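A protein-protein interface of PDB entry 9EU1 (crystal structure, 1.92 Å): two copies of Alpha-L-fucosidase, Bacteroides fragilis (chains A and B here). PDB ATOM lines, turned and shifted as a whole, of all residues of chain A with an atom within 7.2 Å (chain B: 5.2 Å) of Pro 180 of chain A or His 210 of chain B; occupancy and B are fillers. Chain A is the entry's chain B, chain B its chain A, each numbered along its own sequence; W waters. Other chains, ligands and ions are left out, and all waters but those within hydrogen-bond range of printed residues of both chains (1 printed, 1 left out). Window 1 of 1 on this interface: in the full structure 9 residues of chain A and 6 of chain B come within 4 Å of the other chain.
Among the printed residues, pairs that only touch across the chains: Leu 175 of chain A with Arg 211 of chain B (3.4 Å), Gly 179 of chain A with Arg 211 of chain B (3.8 Å), Pro 180 of chain A with His 210 of chain B (3.9 Å), Pro 180 of chain A with Pro 214 of chain B (3.8 Å) and Gln 213 of chain A with Arg 211 of chain B (3.6 Å).
Positions printed for both chains: 213 and 216.
Of the 5 pairs that touch across the chains among the printed residues, none has its exchanged pair printed and touching as well.
Water W1 bridges the guanidinium group of Arg 211 of chain B (2.8 Å) and the backbone carbonyl oxygen of Leu 175 of chain A (2.9 Å).
The side-chain hydroxyl (OH) of Tyr 5 of chain B lies close to a ring nitrogen (NE2) of His 210 of chain B, at 3.3 Å.
O of Pro 214 of chain B sits at hydrogen-bond distance from ND2 of Asn 11 of chain B (3.2 Å).
The backbone carbonyl oxygen (O) of Tyr 206 of chain B lies within hydrogen-bond range of a ring nitrogen (ND1) of His 210 of chain B (3.1 Å).
A ring nitrogen (NE2) of His 210 of chain B is in hydrogen-bond range of the side-chain carboxylate of Asp 231 of chain B (2.7 Å).
The backbone carbonyl oxygen (O) of Leu 175 of chain A lies within hydrogen-bond range of the side-chain amide nitrogen (NE2) of Gln 213 of chain A (2.9 Å).
The backbone carbonyl oxygen of Gly 179 of chain A sits at hydrogen-bond distance from the side-chain amide nitrogen of Gln 213 of chain A.
Of the 16 printed residues of chain B, 3 touch a printed residue of chain A.
Hydrophobic or aromatic side chains of chain B that line the printed part of chain A: Pro 214.
Of the 17 printed residues of chain A, 4 touch a printed residue of chain B.
Printed residues of chain A that touch a printed residue of chain B: Leu 175, Gly 179, Pro 180 and Gln 213.
Hydrophobic or aromatic side chains of chain A that line the printed part of chain B: Pro 180.
Among the printed residues, no Asp or Glu carboxylate lies within 4 Å of a Lys or Arg side-chain nitrogen of the other chain.
Of the printed residues of chain B, Pro 180 of chain A touches His 210 (3.9 Å) and Pro 214 (3.8 Å).
His 210 of chain B touches one residue of chain A.
Printed residues of chain B within 4 Å of Gly 179 of chain A: Arg 211 (3.8 Å).
Of the printed residues of chain B, Gln 213 of chain A touches Arg 211 (3.6 Å).
Leu 208 of chain B touches none of the printed residues of chain A.
The nearest printed residue of chain A that does not touch Arg 211 of chain B is Pro 180 of chain A (4.02 Å).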
ATOM      1  N   ALA A 118      -9.549 -11.231 -11.288  1.00  0.00           N
ATOM      2  CA  ALA A 118      -8.344 -11.263 -12.105  1.00  0.00           C
ATOM      3  C   ALA A 118      -8.275 -12.532 -12.929  1.00  0.00           C
ATOM      4  O   ALA A 118      -7.898 -12.492 -14.109  1.00  0.00           O
ATOM      5  CB  ALA A 118      -7.090 -11.129 -11.229  1.00  0.00           C
ATOM      6  N   ALA A 122      -8.426 -12.895 -17.097  1.00  0.00           N
ATOM      7  CA  ALA A 122      -7.475 -13.576 -17.943  1.00  0.00           C
ATOM      8  C   ALA A 122      -8.193 -14.533 -18.890  1.00  0.00           C
ATOM      9  O   ALA A 122      -7.848 -14.634 -20.078  1.00  0.00           O
ATOM     10  CB  ALA A 122      -6.456 -14.345 -17.087  1.00  0.00           C
ATOM     11  N   ILE A 126      -9.981  -9.664 -20.961  1.00  0.00           N
ATOM     12  CA  ILE A 126     -10.374  -8.334 -20.494  1.00  0.00           C
ATOM     13  C   ILE A 126      -9.263  -7.816 -19.590  1.00  0.00           C
ATOM     14  O   ILE A 126      -8.808  -8.542 -18.700  1.00  0.00           O
ATOM     15  CB  ILE A 126     -11.717  -8.401 -19.752  1.00  0.00           C
ATOM     16  CG1 ILE A 126     -12.803  -8.959 -20.668  1.00  0.00           C
ATOM     17  CG2 ILE A 126     -12.146  -7.005 -19.156  1.00  0.00           C
ATOM     18  CD1 ILE A 126     -13.075  -8.118 -21.918  1.00  0.00           C
ATOM     19  N   LYS A 127      -8.815  -6.583 -19.830  1.00  0.00           N
ATOM     20  CA  LYS A 127      -7.790  -5.965 -18.988  1.00  0.00           C
ATOM     21  C   LYS A 127      -8.407  -5.477 -17.679  1.00  0.00           C
ATOM     22  O   LYS A 127      -9.584  -5.142 -17.618  1.00  0.00           O
ATOM     23  CB  LYS A 127      -7.107  -4.789 -19.683  1.00  0.00           C
ATOM     24  CG  LYS A 127      -6.578  -5.079 -21.096  1.00  0.00           C
ATOM     25  CD  LYS A 127      -5.322  -5.942 -21.092  1.00  0.00           C
ATOM     26  CE  LYS A 127      -4.920  -6.378 -22.513  1.00  0.00           C
ATOM     27  NZ  LYS A 127      -6.015  -7.120 -23.231  1.00  0.00           N
ATOM     28  N   LEU A 128      -7.586  -5.440 -16.629  1.00  0.00           N
ATOM     29  CA  LEU A 128      -8.045  -5.182 -15.268  1.00  0.00           C
ATOM     30  C   LEU A 128      -7.323  -3.953 -14.733  1.00  0.00           C
ATOM     31  O   LEU A 128      -6.080  -3.908 -14.716  1.00  0.00           O
ATOM     32  CB  LEU A 128      -7.788  -6.423 -14.378  1.00  0.00           C
ATOM     33  CG  LEU A 128      -8.203  -6.260 -12.899  1.00  0.00           C
ATOM     34  CD1 LEU A 128      -9.633  -5.845 -12.786  1.00  0.00           C
ATOM     35  CD2 LEU A 128      -8.011  -7.566 -12.175  1.00  0.00           C
ATOM     36  N   HIS A 129      -8.096  -2.934 -14.370  1.00  0.00           N
ATOM     37  CA  HIS A 129      -7.616  -1.709 -13.770  1.00  0.00           C
ATOM     38  C   HIS A 129      -8.089  -1.622 -12.324  1.00  0.00           C
ATOM     39  O   HIS A 129      -9.210  -2.037 -11.994  1.00  0.00           O
ATOM     40  CB  HIS A 129      -8.138  -0.483 -14.515  1.00  0.00           C
ATOM     41  CG  HIS A 129      -7.653  -0.381 -15.917  1.00  0.00           C
ATOM     42  ND1 HIS A 129      -7.867   0.737 -16.693  1.00  0.00           N
ATOM     43  CD2 HIS A 129      -6.945  -1.242 -16.682  1.00  0.00           C
ATOM     44  CE1 HIS A 129      -7.321   0.558 -17.883  1.00  0.00           C
ATOM     45  NE2 HIS A 129      -6.758  -0.637 -17.905  1.00  0.00           N
ATOM     46  N   PHE A 130      -7.248  -1.045 -11.467  1.00  0.00           N
ATOM     47  CA  PHE A 130      -7.583  -0.946 -10.047  1.00  0.00           C
ATOM     48  C   PHE A 130      -7.833   0.511  -9.645  1.00  0.00           C
ATOM     49  O   PHE A 130      -6.956   1.364  -9.780  1.00  0.00           O
ATOM     50  CB  PHE A 130      -6.468  -1.538  -9.202  1.00  0.00           C
ATOM     51  CG  PHE A 130      -6.364  -3.067  -9.241  1.00  0.00           C
ATOM     52  CD1 PHE A 130      -7.429  -3.858  -9.573  1.00  0.00           C
ATOM     53  CD2 PHE A 130      -5.160  -3.682  -8.892  1.00  0.00           C
ATOM     54  CE1 PHE A 130      -7.302  -5.260  -9.564  1.00  0.00           C
ATOM     55  CE2 PHE A 130      -5.032  -5.061  -8.866  1.00  0.00           C
ATOM     56  CZ  PHE A 130      -6.104  -5.856  -9.210  1.00  0.00           C
ATOM     57  N   LEU A 174      -1.131  -5.144  -4.735  1.00  0.00           N
ATOM     58  CA  LEU A 174      -2.016  -5.170  -5.898  1.00  0.00           C
ATOM     59  C   LEU A 174      -1.226  -5.334  -7.186  1.00  0.00           C
ATOM     60  O   LEU A 174      -1.744  -5.886  -8.172  1.00  0.00           O
ATOM     61  CB  LEU A 174      -2.868  -3.893  -5.951  1.00  0.00           C
ATOM     62  CG  LEU A 174      -3.914  -3.735  -4.830  1.00  0.00           C
ATOM     63  CD1 LEU A 174      -4.491  -2.345  -4.815  1.00  0.00           C
ATOM     64  CD2 LEU A 174      -5.047  -4.740  -4.973  1.00  0.00           C
ATOM     65  N   LEU A 175       0.032  -4.885  -7.199  1.00  0.00           N
ATOM     66  CA  LEU A 175       0.847  -4.923  -8.402  1.00  0.00           C
ATOM     67  C   LEU A 175       1.805  -6.112  -8.447  1.00  0.00           C
ATOM     68  O   LEU A 175       2.604  -6.212  -9.381  1.00  0.00           O
ATOM     69  CB  LEU A 175       1.649  -3.616  -8.541  1.00  0.00           C
ATOM     70  CG  LEU A 175       0.750  -2.394  -8.824  1.00  0.00           C
ATOM     71  CD1 LEU A 175       1.513  -1.084  -8.636  1.00  0.00           C
ATOM     72  CD2 LEU A 175       0.201  -2.500 -10.244  1.00  0.00           C
ATOM     73  N   TYR A 178      -1.663 -10.188  -8.388  1.00  0.00           N
ATOM     74  CA  TYR A 178      -2.890 -10.269  -9.170  1.00  0.00           C
ATOM     75  C   TYR A 178      -2.617 -10.198 -10.668  1.00  0.00           C
ATOM     76  O   TYR A 178      -3.468  -9.744 -11.438  1.00  0.00           O
ATOM     77  CB  TYR A 178      -3.881  -9.163  -8.763  1.00  0.00           C
ATOM     78  CG  TYR A 178      -4.298  -9.273  -7.318  1.00  0.00           C
ATOM     79  CD1 TYR A 178      -5.279 -10.160  -6.931  1.00  0.00           C
ATOM     80  CD2 TYR A 178      -3.629  -8.549  -6.319  1.00  0.00           C
ATOM     81  CE1 TYR A 178      -5.644 -10.298  -5.586  1.00  0.00           C
ATOM     82  CE2 TYR A 178      -3.974  -8.690  -4.989  1.00  0.00           C
ATOM     83  CZ  TYR A 178      -4.976  -9.572  -4.630  1.00  0.00           C
ATOM     84  OH  TYR A 178      -5.323  -9.716  -3.315  1.00  0.00           O
ATOM     85  N   GLY A 179      -1.441 -10.646 -11.095  1.00  0.00           N
ATOM     86  CA  GLY A 179      -1.103 -10.687 -12.501  1.00  0.00           C
ATOM     87  C   GLY A 179      -0.913  -9.303 -13.101  1.00  0.00           C
ATOM     88  O   GLY A 179      -0.719  -8.313 -12.386  1.00  0.00           O
ATOM     89  N   PRO A 180      -0.931  -9.220 -14.434  1.00  0.00           N
ATOM     90  CA  PRO A 180      -0.711  -7.931 -15.099  1.00  0.00           C
ATOM     91  C   PRO A 180      -1.889  -6.993 -14.870  1.00  0.00           C
ATOM     92  O   PRO A 180      -3.048  -7.358 -15.091  1.00  0.00           O
ATOM     93  CB  PRO A 180      -0.597  -8.305 -16.588  1.00  0.00           C
ATOM     94  CG  PRO A 180      -0.750  -9.758 -16.659  1.00  0.00           C
ATOM     95  CD  PRO A 180      -1.380 -10.234 -15.399  1.00  0.00           C
ATOM     96  N   ILE A 181      -1.580  -5.759 -14.466  1.00  0.00           N
ATOM     97  CA  ILE A 181      -2.589  -4.740 -14.171  1.00  0.00           C
ATOM     98  C   ILE A 181      -2.428  -3.594 -15.170  1.00  0.00           C
ATOM     99  O   ILE A 181      -1.327  -3.050 -15.325  1.00  0.00           O
ATOM    100  CB  ILE A 181      -2.448  -4.229 -12.725  1.00  0.00           C
ATOM    101  CG1 ILE A 181      -2.642  -5.387 -11.730  1.00  0.00           C
ATOM    102  CG2 ILE A 181      -3.416  -3.080 -12.470  1.00  0.00           C
ATOM    103  CD1 ILE A 181      -3.993  -6.127 -11.867  1.00  0.00           C
ATOM    104  N   GLY A 182      -3.516  -3.251 -15.860  1.00  0.00           N
ATOM    105  CA  GLY A 182      -3.455  -2.219 -16.887  1.00  0.00           C
ATOM    106  C   GLY A 182      -3.375  -0.799 -16.378  1.00  0.00           C
ATOM    107  O   GLY A 182      -2.862   0.081 -17.087  1.00  0.00           O
ATOM    108  N   ALA A 183      -3.878  -0.535 -15.173  1.00  0.00           N
ATOM    109  CA  ALA A 183      -3.806   0.828 -14.645  1.00  0.00           C
ATOM    110  C   ALA A 183      -4.108   0.861 -13.154  1.00  0.00           C
ATOM    111  O   ALA A 183      -4.853   0.035 -12.637  1.00  0.00           O
ATOM    112  CB  ALA A 183      -4.809   1.750 -15.372  1.00  0.00           C
ATOM    113  N   GLN A 213       5.418  -2.645 -12.203  1.00  0.00           N
ATOM    114  CA  GLN A 213       4.950  -2.980 -13.547  1.00  0.00           C
ATOM    115  C   GLN A 213       5.091  -1.776 -14.484  1.00  0.00           C
ATOM    116  O   GLN A 213       4.182  -0.924 -14.564  1.00  0.00           O
ATOM    117  CB  GLN A 213       3.502  -3.459 -13.532  1.00  0.00           C
ATOM    118  CG  GLN A 213       3.224  -4.643 -12.632  1.00  0.00           C
ATOM    119  CD  GLN A 213       1.867  -5.273 -12.911  1.00  0.00           C
ATOM    120  OE1 GLN A 213       1.330  -5.155 -14.015  1.00  0.00           O
ATOM    121  NE2 GLN A 213       1.296  -5.933 -11.900  1.00  0.00           N
ATOM    122  N   CYS A 216       2.068  -0.588 -16.490  1.00  0.00           N
ATOM    123  CA  CYS A 216       0.849  -0.137 -15.830  1.00  0.00           C
ATOM    124  C   CYS A 216       0.681   1.362 -15.997  1.00  0.00           C
ATOM    125  O   CYS A 216       1.635   2.123 -15.865  1.00  0.00           O
ATOM    126  CB  CYS A 216       0.885  -0.495 -14.340  1.00  0.00           C
ATOM    127  SG  CYS A 216      -0.606  -0.132 -13.453  1.00  0.00           S
ATOM    128  N   TYR B   5      -4.183 -21.897 -13.458  1.00  0.00           N
ATOM    129  CA  TYR B   5      -3.470 -21.155 -14.495  1.00  0.00           C
ATOM    130  C   TYR B   5      -4.356 -20.970 -15.718  1.00  0.00           C
ATOM    131  O   TYR B   5      -4.836 -21.954 -16.293  1.00  0.00           O
ATOM    132  CB  TYR B   5      -2.192 -21.873 -14.917  1.00  0.00           C
ATOM    133  CG  TYR B   5      -1.416 -21.119 -15.989  1.00  0.00           C
ATOM    134  CD1 TYR B   5      -1.001 -19.806 -15.793  1.00  0.00           C
ATOM    135  CD2 TYR B   5      -1.126 -21.711 -17.196  1.00  0.00           C
ATOM    136  CE1 TYR B   5      -0.301 -19.131 -16.774  1.00  0.00           C
ATOM    137  CE2 TYR B   5      -0.424 -21.036 -18.190  1.00  0.00           C
ATOM    138  CZ  TYR B   5      -0.031 -19.748 -17.971  1.00  0.00           C
ATOM    139  OH  TYR B   5       0.659 -19.096 -18.977  1.00  0.00           O
ATOM    140  N   ASN B  11      -0.507 -14.581 -24.269  1.00  0.00           N
ATOM    141  CA  ASN B  11       0.325 -15.777 -24.209  1.00  0.00           C
ATOM    142  C   ASN B  11      -0.084 -16.792 -25.276  1.00  0.00           C
ATOM    143  O   ASN B  11       0.776 -17.380 -25.949  1.00  0.00           O
ATOM    144  CB  ASN B  11       0.260 -16.399 -22.826  1.00  0.00           C
ATOM    145  CG  ASN B  11       1.401 -17.414 -22.606  1.00  0.00           C
ATOM    146  OD1 ASN B  11       1.255 -18.598 -22.893  1.00  0.00           O
ATOM    147  ND2 ASN B  11       2.531 -16.926 -22.120  1.00  0.00           N
ATOM    148  N   TYR B 206       6.774 -18.523 -12.047  1.00  0.00           N
ATOM    149  CA  TYR B 206       6.110 -18.413 -13.345  1.00  0.00           C
ATOM    150  C   TYR B 206       5.179 -17.190 -13.384  1.00  0.00           C
ATOM    151  O   TYR B 206       5.050 -16.514 -14.421  1.00  0.00           O
ATOM    152  CB  TYR B 206       5.297 -19.677 -13.608  1.00  0.00           C
ATOM    153  CG  TYR B 206       6.110 -20.952 -13.768  1.00  0.00           C
ATOM    154  CD1 TYR B 206       7.501 -20.933 -13.827  1.00  0.00           C
ATOM    155  CD2 TYR B 206       5.474 -22.162 -13.872  1.00  0.00           C
ATOM    156  CE1 TYR B 206       8.226 -22.099 -14.024  1.00  0.00           C
ATOM    157  CE2 TYR B 206       6.181 -23.327 -14.043  1.00  0.00           C
ATOM    158  CZ  TYR B 206       7.549 -23.295 -14.127  1.00  0.00           C
ATOM    159  OH  TYR B 206       8.218 -24.477 -14.292  1.00  0.00           O
ATOM    160  N   ALA B 207       4.497 -16.923 -12.273  1.00  0.00           N
ATOM    161  CA  ALA B 207       3.595 -15.769 -12.212  1.00  0.00           C
ATOM    162  C   ALA B 207       4.368 -14.465 -12.374  1.00  0.00           C
ATOM    163  O   ALA B 207       3.892 -13.532 -13.019  1.00  0.00           O
ATOM    164  CB  ALA B 207       2.844 -15.760 -10.885  1.00  0.00           C
ATOM    165  N   LEU B 208       5.578 -14.392 -11.792  1.00  0.00           N
ATOM    166  CA  LEU B 208       6.394 -13.190 -11.960  1.00  0.00           C
ATOM    167  C   LEU B 208       6.690 -12.945 -13.429  1.00  0.00           C
ATOM    168  O   LEU B 208       6.573 -11.816 -13.926  1.00  0.00           O
ATOM    169  CB  LEU B 208       7.691 -13.330 -11.175  1.00  0.00           C
ATOM    170  CG  LEU B 208       8.769 -12.263 -11.336  1.00  0.00           C
ATOM    171  CD1 LEU B 208       9.688 -12.293 -10.115  1.00  0.00           C
ATOM    172  CD2 LEU B 208       9.615 -12.435 -12.586  1.00  0.00           C
ATOM    173  N   ILE B 209       7.056 -14.008 -14.155  1.00  0.00           N
ATOM    174  CA  ILE B 209       7.384 -13.864 -15.570  1.00  0.00           C
ATOM    175  C   ILE B 209       6.173 -13.374 -16.341  1.00  0.00           C
ATOM    176  O   ILE B 209       6.271 -12.462 -17.177  1.00  0.00           O
ATOM    177  CB  ILE B 209       7.911 -15.209 -16.120  1.00  0.00           C
ATOM    178  CG1 ILE B 209       9.232 -15.542 -15.422  1.00  0.00           C
ATOM    179  CG2 ILE B 209       7.998 -15.129 -17.646  1.00  0.00           C
ATOM    180  CD1 ILE B 209       9.772 -16.965 -15.660  1.00  0.00           C
ATOM    181  N   HIS B 210       5.013 -14.001 -16.102  1.00  0.00           N
ATOM    182  CA  HIS B 210       3.812 -13.642 -16.844  1.00  0.00           C
ATOM    183  C   HIS B 210       3.296 -12.273 -16.418  1.00  0.00           C
ATOM    184  O   HIS B 210       2.613 -11.600 -17.196  1.00  0.00           O
ATOM    185  CB  HIS B 210       2.734 -14.674 -16.632  1.00  0.00           C
ATOM    186  CG  HIS B 210       3.057 -16.004 -17.234  1.00  0.00           C
ATOM    187  ND1 HIS B 210       2.909 -17.184 -16.539  1.00  0.00           N
ATOM    188  CD2 HIS B 210       3.495 -16.339 -18.470  1.00  0.00           C
ATOM    189  CE1 HIS B 210       3.235 -18.196 -17.328  1.00  0.00           C
ATOM    190  NE2 HIS B 210       3.606 -17.710 -18.500  1.00  0.00           N
ATOM    191  N   ARG B 211       3.586 -11.875 -15.180  1.00  0.00           N
ATOM    192  CA  ARG B 211       3.172 -10.541 -14.733  1.00  0.00           C
ATOM    193  C   ARG B 211       3.947  -9.455 -15.476  1.00  0.00           C
ATOM    194  O   ARG B 211       3.362  -8.474 -15.915  1.00  0.00           O
ATOM    195  CB  ARG B 211       3.365 -10.418 -13.226  1.00  0.00           C
ATOM    196  CG  ARG B 211       2.976  -9.050 -12.678  1.00  0.00           C
ATOM    197  CD  ARG B 211       2.937  -9.094 -11.162  1.00  0.00           C
ATOM    198  NE  ARG B 211       4.259  -9.340 -10.592  1.00  0.00           N
ATOM    199  CZ  ARG B 211       4.625 -10.474 -10.013  1.00  0.00           C
ATOM    200  NH1 ARG B 211       3.833 -11.537  -9.995  1.00  0.00           N
ATOM    201  NH2 ARG B 211       5.827 -10.550  -9.442  1.00  0.00           N
ATOM    202  N   LEU B 212       5.259  -9.635 -15.653  1.00  0.00           N
ATOM    203  CA  LEU B 212       6.082  -8.587 -16.263  1.00  0.00           C
ATOM    204  C   LEU B 212       5.998  -8.605 -17.777  1.00  0.00           C
ATOM    205  O   LEU B 212       6.016  -7.545 -18.413  1.00  0.00           O
ATOM    206  CB  LEU B 212       7.531  -8.726 -15.848  1.00  0.00           C
ATOM    207  CG  LEU B 212       7.790  -8.660 -14.341  1.00  0.00           C
ATOM    208  CD1 LEU B 212       9.288  -8.721 -14.086  1.00  0.00           C
ATOM    209  CD2 LEU B 212       7.148  -7.390 -13.772  1.00  0.00           C
ATOM    210  N   GLN B 213       5.866  -9.783 -18.374  1.00  0.00           N
ATOM    211  CA  GLN B 213       5.728  -9.887 -19.833  1.00  0.00           C
ATOM    212  C   GLN B 213       4.730 -10.989 -20.131  1.00  0.00           C
ATOM    213  O   GLN B 213       5.104 -12.170 -20.226  1.00  0.00           O
ATOM    214  CB  GLN B 213       7.072 -10.169 -20.491  1.00  0.00           C
ATOM    215  CG  GLN B 213       8.003  -8.945 -20.499  1.00  0.00           C
ATOM    216  CD  GLN B 213       9.127  -9.075 -21.518  1.00  0.00           C
ATOM    217  OE1 GLN B 213       8.946  -9.689 -22.576  1.00  0.00           O
ATOM    218  NE2 GLN B 213      10.269  -8.494 -21.212  1.00  0.00           N
ATOM    219  N   PRO B 214       3.437 -10.641 -20.227  1.00  0.00           N
ATOM    220  CA  PRO B 214       2.417 -11.668 -20.469  1.00  0.00           C
ATOM    221  C   PRO B 214       2.693 -12.547 -21.676  1.00  0.00           C
ATOM    222  O   PRO B 214       2.363 -13.735 -21.622  1.00  0.00           O
ATOM    223  CB  PRO B 214       1.118 -10.852 -20.665  1.00  0.00           C
ATOM    224  CG  PRO B 214       1.364  -9.584 -19.809  1.00  0.00           C
ATOM    225  CD  PRO B 214       2.852  -9.306 -19.923  1.00  0.00           C
ATOM    226  N   CYS B 216       5.522 -13.623 -22.720  1.00  0.00           N
ATOM    227  CA  CYS B 216       6.712 -14.471 -22.561  1.00  0.00           C
ATOM    228  C   CYS B 216       6.309 -15.904 -22.228  1.00  0.00           C
ATOM    229  O   CYS B 216       5.484 -16.140 -21.323  1.00  0.00           O
ATOM    230  CB  CYS B 216       7.606 -13.917 -21.459  1.00  0.00           C
ATOM    231  SG  CYS B 216       9.166 -14.781 -21.289  1.00  0.00           S
ATOM    232  N   LEU B 217       6.878 -16.856 -22.950  1.00  0.00           N
ATOM    233  CA  LEU B 217       6.584 -18.264 -22.742  1.00  0.00           C
ATOM    234  C   LEU B 217       7.499 -18.862 -21.671  1.00  0.00           C
ATOM    235  O   LEU B 217       8.683 -18.534 -21.579  1.00  0.00           O
ATOM    236  CB  LEU B 217       6.743 -19.035 -24.060  1.00  0.00           C
ATOM    237  CG  LEU B 217       5.947 -18.546 -25.270  1.00  0.00           C
ATOM    238  CD1 LEU B 217       6.394 -19.230 -26.543  1.00  0.00           C
ATOM    239  CD2 LEU B 217       4.448 -18.783 -25.058  1.00  0.00           C
ATOM    240  N   VAL B 218       6.948 -19.754 -20.856  1.00  0.00           N
ATOM    241  CA  VAL B 218       7.706 -20.407 -19.791  1.00  0.00           C
ATOM    242  C   VAL B 218       7.938 -21.867 -20.166  1.00  0.00           C
ATOM    243  O   VAL B 218       6.992 -22.595 -20.487  1.00  0.00           O
ATOM    244  CB  VAL B 218       6.974 -20.291 -18.440  1.00  0.00           C
ATOM    245  CG1 VAL B 218       7.607 -21.150 -17.426  1.00  0.00           C
ATOM    246  CG2 VAL B 218       6.987 -18.829 -17.983  1.00  0.00           C
ATOM    247  N   GLY B 229       1.357 -23.402 -15.436  1.00  0.00           N
ATOM    248  CA  GLY B 229       2.117 -22.191 -15.627  1.00  0.00           C
ATOM    249  C   GLY B 229       3.157 -22.251 -16.746  1.00  0.00           C
ATOM    250  O   GLY B 229       3.597 -21.194 -17.222  1.00  0.00           O
ATOM    251  N   ASP B 231       4.235 -22.854 -20.643  1.00  0.00           N
ATOM    252  CA  ASP B 231       3.631 -22.592 -21.931  1.00  0.00           C
ATOM    253  C   ASP B 231       4.222 -23.403 -23.077  1.00  0.00           C
ATOM    254  O   ASP B 231       3.626 -23.421 -24.164  1.00  0.00           O
ATOM    255  CB  ASP B 231       3.757 -21.097 -22.263  1.00  0.00           C
ATOM    256  CG  ASP B 231       3.216 -20.227 -21.143  1.00  0.00           C
ATOM    257  OD1 ASP B 231       2.069 -20.501 -20.714  1.00  0.00           O
ATOM    258  OD2 ASP B 231       3.959 -19.341 -20.669  1.00  0.00           O
HETATM  259  O   HOH W   1       5.333  -6.818 -10.228  1.00  0.00           O
